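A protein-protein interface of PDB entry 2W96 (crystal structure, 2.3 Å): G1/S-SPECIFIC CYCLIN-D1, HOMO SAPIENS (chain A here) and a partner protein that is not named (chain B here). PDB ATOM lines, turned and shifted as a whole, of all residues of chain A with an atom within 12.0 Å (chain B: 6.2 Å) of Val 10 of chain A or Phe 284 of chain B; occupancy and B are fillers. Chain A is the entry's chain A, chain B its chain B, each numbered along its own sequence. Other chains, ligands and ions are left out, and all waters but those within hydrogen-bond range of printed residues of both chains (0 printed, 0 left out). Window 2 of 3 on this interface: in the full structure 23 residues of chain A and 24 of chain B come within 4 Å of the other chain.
The side-chain carboxylate (OE1) of Glu 9 of chain A sits close to the side-chain hydroxyl (OG) of Ser 282 of chain B, 3.4 Å away.
The guanidinium group (NE) of Arg 285 of chain B lies within salt-bridge range of the side-chain carboxylate (OE2) of Glu 9 of chain A, 2.6 Å away.
Along chain A the printed residues that touch a printed residue of chain B span positions 9 to 13.
Printed residues of chain B that touch a printed residue of chain A: Asp 126, Ser 282, Phe 284 and Arg 285.
Phe 284 of chain B touches Val 10 of chain A (CD2 to CG2, 3.1 Å).
O of Ile 13 of chain A touches OD2 of Asp 126 of chain B (3.7 Å).
Ile 13 of chain A touches Phe 284 of chain B.
Val 10 of chain A touches just one residue of chain B: Phe 284 (3.1 Å).
Phe 284 of chain B touches two residues of chain A.
No residue of chain A comes within 4 Å of Ala 283 of chain B.
No residue of chain A comes within 4 Å of Leu 287 of chain B.
No residue of chain A comes within 4 Å of Gln 288 of chain B.
Printed residues of chain B within 4 Å of Glu 9 of chain A: Ser 282 and Arg 285.
Of the printed residues of chain B, Ile 13 of chain A touches Asp 126 (3.7 Å) and Phe 284 (3.0 Å).
The nearest residue of chain B that does not touch Val 10 of chain A is Arg 285 of chain B (5.8 Å).
The nearest residue of chain A that does not touch Phe 284 of chain B is Thr 12 of chain A (4.2 Å).
The guanidinium group (NE) of Arg 285 of chain B sits at hydrogen-bond distance from the side-chain hydroxyl (OG) of Ser 282 of chain B (3.0 Å).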
ATOM      1  N   LEU A   6     -26.610  33.222  11.250  1.00  0.00           N
ATOM      2  CA  LEU A   6     -25.996  32.004  10.733  1.00  0.00           C
ATOM      3  C   LEU A   6     -24.501  32.109  10.969  1.00  0.00           C
ATOM      4  O   LEU A   6     -23.764  32.637  10.137  1.00  0.00           O
ATOM      5  CB  LEU A   6     -26.297  31.838   9.241  1.00  0.00           C
ATOM      6  CG  LEU A   6     -27.531  32.598   8.751  1.00  0.00           C
ATOM      7  CD1 LEU A   6     -27.177  34.046   8.486  1.00  0.00           C
ATOM      8  CD2 LEU A   6     -28.159  31.967   7.525  1.00  0.00           C
ATOM      9  N   CYS A   7     -24.053  31.568  12.094  1.00  0.00           N
ATOM     10  CA  CYS A   7     -22.766  31.946  12.651  1.00  0.00           C
ATOM     11  C   CYS A   7     -21.554  31.069  12.313  1.00  0.00           C
ATOM     12  O   CYS A   7     -21.147  30.220  13.107  1.00  0.00           O
ATOM     13  CB  CYS A   7     -22.908  32.208  14.148  1.00  0.00           C
ATOM     14  SG  CYS A   7     -24.246  33.375  14.499  1.00  0.00           S
ATOM     15  N   CYS A   8     -20.952  31.350  11.156  1.00  0.00           N
ATOM     16  CA  CYS A   8     -19.588  30.932  10.810  1.00  0.00           C
ATOM     17  C   CYS A   8     -18.666  30.863  12.020  1.00  0.00           C
ATOM     18  O   CYS A   8     -18.939  31.468  13.055  1.00  0.00           O
ATOM     19  CB  CYS A   8     -18.972  31.906   9.792  1.00  0.00           C
ATOM     20  SG  CYS A   8     -19.489  31.703   8.076  1.00  0.00           S
ATOM     21  N   GLU A   9     -17.530  30.198  11.854  1.00  0.00           N
ATOM     22  CA  GLU A   9     -16.481  30.248  12.865  1.00  0.00           C
ATOM     23  C   GLU A   9     -15.385  31.254  12.537  1.00  0.00           C
ATOM     24  O   GLU A   9     -14.583  31.609  13.400  1.00  0.00           O
ATOM     25  CB  GLU A   9     -15.877  28.869  13.117  1.00  0.00           C
ATOM     26  CG  GLU A   9     -14.692  28.902  14.065  1.00  0.00           C
ATOM     27  CD  GLU A   9     -14.731  27.784  15.086  1.00  0.00           C
ATOM     28  OE1 GLU A   9     -15.843  27.382  15.489  1.00  0.00           O
ATOM     29  OE2 GLU A   9     -13.649  27.347  15.526  1.00  0.00           O
ATOM     30  N   VAL A  10     -15.361  31.736  11.300  1.00  0.00           N
ATOM     31  CA  VAL A  10     -14.335  32.690  10.902  1.00  0.00           C
ATOM     32  C   VAL A  10     -14.863  34.064  10.473  1.00  0.00           C
ATOM     33  O   VAL A  10     -15.523  34.770  11.242  1.00  0.00           O
ATOM     34  CB  VAL A  10     -13.380  32.083   9.851  1.00  0.00           C
ATOM     35  CG1 VAL A  10     -12.257  33.051   9.506  1.00  0.00           C
ATOM     36  CG2 VAL A  10     -12.808  30.761  10.351  1.00  0.00           C
ATOM     37  N   GLU A  11     -14.648  34.378   9.201  1.00  0.00           N
ATOM     38  CA  GLU A  11     -14.499  35.755   8.748  1.00  0.00           C
ATOM     39  C   GLU A  11     -13.777  35.629   7.407  1.00  0.00           C
ATOM     40  O   GLU A  11     -13.267  36.605   6.854  1.00  0.00           O
ATOM     41  CB  GLU A  11     -13.644  36.522   9.762  1.00  0.00           C
ATOM     42  CG  GLU A  11     -13.198  37.914   9.353  1.00  0.00           C
ATOM     43  CD  GLU A  11     -11.940  38.329  10.090  1.00  0.00           C
ATOM     44  OE1 GLU A  11     -11.198  37.422  10.527  1.00  0.00           O
ATOM     45  OE2 GLU A  11     -11.686  39.545  10.229  1.00  0.00           O
ATOM     46  N   THR A  12     -13.582  34.373   7.016  1.00  0.00           N
ATOM     47  CA  THR A  12     -13.367  33.975   5.629  1.00  0.00           C
ATOM     48  C   THR A  12     -14.464  32.939   5.379  1.00  0.00           C
ATOM     49  O   THR A  12     -14.849  32.682   4.236  1.00  0.00           O
ATOM     50  CB  THR A  12     -11.970  33.337   5.430  1.00  0.00           C
ATOM     51  OG1 THR A  12     -11.095  33.739   6.493  1.00  0.00           O
ATOM     52  CG2 THR A  12     -11.376  33.759   4.085  1.00  0.00           C
ATOM     53  N   ILE A  13     -14.945  32.367   6.487  1.00  0.00           N
ATOM     54  CA  ILE A  13     -16.056  31.413   6.551  1.00  0.00           C
ATOM     55  C   ILE A  13     -15.621  29.965   6.714  1.00  0.00           C
ATOM     56  O   ILE A  13     -16.399  29.128   7.174  1.00  0.00           O
ATOM     57  CB  ILE A  13     -17.045  31.559   5.396  1.00  0.00           C
ATOM     58  N   ARG A  26     -22.667  36.056   1.195  1.00  0.00           N
ATOM     59  CA  ARG A  26     -22.866  34.612   1.144  1.00  0.00           C
ATOM     60  C   ARG A  26     -24.143  34.299   1.915  1.00  0.00           C
ATOM     61  O   ARG A  26     -24.874  33.362   1.584  1.00  0.00           O
ATOM     62  CB  ARG A  26     -21.676  33.877   1.769  1.00  0.00           C
ATOM     63  CG  ARG A  26     -20.308  34.378   1.315  1.00  0.00           C
ATOM     64  CD  ARG A  26     -20.079  34.198  -0.184  1.00  0.00           C
ATOM     65  NE  ARG A  26     -20.103  32.797  -0.601  1.00  0.00           N
ATOM     66  CZ  ARG A  26     -20.975  32.289  -1.469  1.00  0.00           C
ATOM     67  NH1 ARG A  26     -21.890  33.070  -2.029  1.00  0.00           N
ATOM     68  NH2 ARG A  26     -20.923  31.003  -1.791  1.00  0.00           N
ATOM     69  N   VAL A  27     -24.417  35.127   2.921  1.00  0.00           N
ATOM     70  CA  VAL A  27     -25.626  35.016   3.737  1.00  0.00           C
ATOM     71  C   VAL A  27     -26.857  35.427   2.937  1.00  0.00           C
ATOM     72  O   VAL A  27     -27.795  34.643   2.772  1.00  0.00           O
ATOM     73  CB  VAL A  27     -25.503  35.862   5.027  1.00  0.00           C
ATOM     74  CG1 VAL A  27     -24.932  37.235   4.706  1.00  0.00           C
ATOM     75  CG2 VAL A  27     -26.856  35.994   5.711  1.00  0.00           C
ATOM     76  N   LEU B 122     -15.884  17.375   6.410  1.00  0.00           N
ATOM     77  CA  LEU B 122     -15.678  18.642   7.104  1.00  0.00           C
ATOM     78  C   LEU B 122     -16.450  19.781   6.439  1.00  0.00           C
ATOM     79  O   LEU B 122     -16.889  20.710   7.111  1.00  0.00           O
ATOM     80  CB  LEU B 122     -14.189  18.997   7.172  1.00  0.00           C
ATOM     81  CG  LEU B 122     -13.257  18.111   8.003  1.00  0.00           C
ATOM     82  CD1 LEU B 122     -11.836  18.643   7.954  1.00  0.00           C
ATOM     83  CD2 LEU B 122     -13.742  18.014   9.441  1.00  0.00           C
ATOM     84  N   ASP B 126     -19.082  21.688   8.516  1.00  0.00           N
ATOM     85  CA  ASP B 126     -18.887  23.137   8.572  1.00  0.00           C
ATOM     86  C   ASP B 126     -20.186  23.878   8.221  1.00  0.00           C
ATOM     87  O   ASP B 126     -20.563  24.848   8.881  1.00  0.00           O
ATOM     88  CB  ASP B 126     -17.760  23.531   7.605  1.00  0.00           C
ATOM     89  CG  ASP B 126     -17.473  25.027   7.601  1.00  0.00           C
ATOM     90  OD1 ASP B 126     -17.343  25.620   8.689  1.00  0.00           O
ATOM     91  OD2 ASP B 126     -17.301  25.593   6.505  1.00  0.00           O
ATOM     92  N   MET B 194     -16.542  17.225  16.091  1.00  0.00           N
ATOM     93  CA  MET B 194     -15.165  17.130  15.620  1.00  0.00           C
ATOM     94  C   MET B 194     -14.407  15.983  16.285  1.00  0.00           C
ATOM     95  O   MET B 194     -13.569  15.341  15.658  1.00  0.00           O
ATOM     96  CB  MET B 194     -14.431  18.459  15.811  1.00  0.00           C
ATOM     97  CG  MET B 194     -14.942  19.571  14.911  1.00  0.00           C
ATOM     98  SD  MET B 194     -14.925  19.117  13.162  1.00  0.00           S
ATOM     99  CE  MET B 194     -13.142  18.917  12.853  1.00  0.00           C
ATOM    100  N   SER B 282     -11.647  22.952  14.840  1.00  0.00           N
ATOM    101  CA  SER B 282     -12.962  23.068  14.219  1.00  0.00           C
ATOM    102  C   SER B 282     -12.980  22.466  12.818  1.00  0.00           C
ATOM    103  O   SER B 282     -11.955  21.997  12.316  1.00  0.00           O
ATOM    104  CB  SER B 282     -13.388  24.531  14.164  1.00  0.00           C
ATOM    105  OG  SER B 282     -13.399  25.086  15.465  1.00  0.00           O
ATOM    106  N   ALA B 283     -14.151  22.474  12.191  1.00  0.00           N
ATOM    107  CA  ALA B 283     -14.309  21.867  10.876  1.00  0.00           C
ATOM    108  C   ALA B 283     -13.737  22.760   9.782  1.00  0.00           C
ATOM    109  O   ALA B 283     -13.403  22.288   8.696  1.00  0.00           O
ATOM    110  CB  ALA B 283     -15.773  21.552  10.606  1.00  0.00           C
ATOM    111  N   PHE B 284     -13.625  24.052  10.075  1.00  0.00           N
ATOM    112  CA  PHE B 284     -13.028  24.995   9.136  1.00  0.00           C
ATOM    113  C   PHE B 284     -11.511  25.083   9.303  1.00  0.00           C
ATOM    114  O   PHE B 284     -10.779  25.146   8.317  1.00  0.00           O
ATOM    115  CB  PHE B 284     -13.660  26.382   9.272  1.00  0.00           C
ATOM    116  CG  PHE B 284     -13.132  27.386   8.286  1.00  0.00           C
ATOM    117  CD1 PHE B 284     -13.645  27.454   7.004  1.00  0.00           C
ATOM    118  CD2 PHE B 284     -12.106  28.250   8.638  1.00  0.00           C
ATOM    119  CE1 PHE B 284     -13.156  28.373   6.092  1.00  0.00           C
ATOM    120  CE2 PHE B 284     -11.615  29.174   7.730  1.00  0.00           C
ATOM    121  CZ  PHE B 284     -12.142  29.234   6.454  1.00  0.00           C
ATOM    122  N   ARG B 285     -11.053  25.105  10.553  1.00  0.00           N
ATOM    123  CA  ARG B 285      -9.620  25.119  10.851  1.00  0.00           C
ATOM    124  C   ARG B 285      -9.003  23.809  10.386  1.00  0.00           C
ATOM    125  O   ARG B 285      -7.855  23.776   9.934  1.00  0.00           O
ATOM    126  CB  ARG B 285      -9.372  25.274  12.354  1.00  0.00           C
ATOM    127  CG  ARG B 285     -10.319  26.224  13.067  1.00  0.00           C
ATOM    128  CD  ARG B 285     -10.090  26.176  14.571  1.00  0.00           C
ATOM    129  NE  ARG B 285     -11.079  26.957  15.309  1.00  0.00           N
ATOM    130  CZ  ARG B 285     -11.147  27.014  16.636  1.00  0.00           C
ATOM    131  NH1 ARG B 285     -12.086  27.747  17.220  1.00  0.00           N
ATOM    132  NH2 ARG B 285     -10.285  26.331  17.378  1.00  0.00           N
ATOM    133  N   ALA B 286      -9.759  22.725  10.552  1.00  0.00           N
ATOM    134  CA  ALA B 286      -9.348  21.405  10.086  1.00  0.00           C
ATOM    135  C   ALA B 286      -9.209  21.382   8.567  1.00  0.00           C
ATOM    136  O   ALA B 286      -8.186  20.955   8.033  1.00  0.00           O
ATOM    137  CB  ALA B 286     -10.341  20.357  10.545  1.00  0.00           C
ATOM    138  N   LEU B 287     -10.240  21.859   7.877  1.00  0.00           N
ATOM    139  CA  LEU B 287     -10.228  21.939   6.418  1.00  0.00           C
ATOM    140  C   LEU B 287      -8.983  22.657   5.917  1.00  0.00           C
ATOM    141  O   LEU B 287      -8.465  22.359   4.839  1.00  0.00           O
ATOM    142  CB  LEU B 287     -11.483  22.655   5.916  1.00  0.00           C
ATOM    143  CG  LEU B 287     -12.760  21.821   5.834  1.00  0.00           C
ATOM    144  CD1 LEU B 287     -13.973  22.732   5.742  1.00  0.00           C
ATOM    145  CD2 LEU B 287     -12.699  20.895   4.628  1.00  0.00           C
ATOM    146  N   GLN B 288      -8.517  23.618   6.704  1.00  0.00           N
ATOM    147  CA  GLN B 288      -7.319  24.370   6.361  1.00  0.00           C
ATOM    148  C   GLN B 288      -6.092  23.785   7.055  1.00  0.00           C
ATOM    149  O   GLN B 288      -5.339  24.498   7.721  1.00  0.00           O
ATOM    150  CB  GLN B 288      -7.498  25.844   6.719  1.00  0.00           C
ATOM    151  CG  GLN B 288      -8.643  26.515   5.982  1.00  0.00           C
ATOM    152  CD  GLN B 288      -8.642  28.016   6.159  1.00  0.00           C
ATOM    153  OE1 GLN B 288      -8.340  28.523   7.240  1.00  0.00           O
ATOM    154  NE2 GLN B 288      -8.957  28.740   5.091  1.00  0.00           N
ATOM    155  N   HIS B 289      -5.922  22.474   6.922  1.00  0.00           N
ATOM    156  CA  HIS B 289      -4.769  21.782   7.484  1.00  0.00           C
ATOM    157  C   HIS B 289      -3.853  21.292   6.364  1.00  0.00           C
ATOM    158  O   HIS B 289      -4.309  21.020   5.251  1.00  0.00           O
ATOM    159  CB  HIS B 289      -5.221  20.603   8.357  1.00  0.00           C
ATOM    160  CG  HIS B 289      -4.120  19.994   9.169  1.00  0.00           C
ATOM    161  ND1 HIS B 289      -3.553  18.772   8.865  1.00  0.00           N
ATOM    162  CD2 HIS B 289      -3.489  20.428  10.287  1.00  0.00           C
ATOM    163  CE1 HIS B 289      -2.620  18.487   9.752  1.00  0.00           C
ATOM    164  NE2 HIS B 289      -2.560  19.477  10.628  1.00  0.00           N
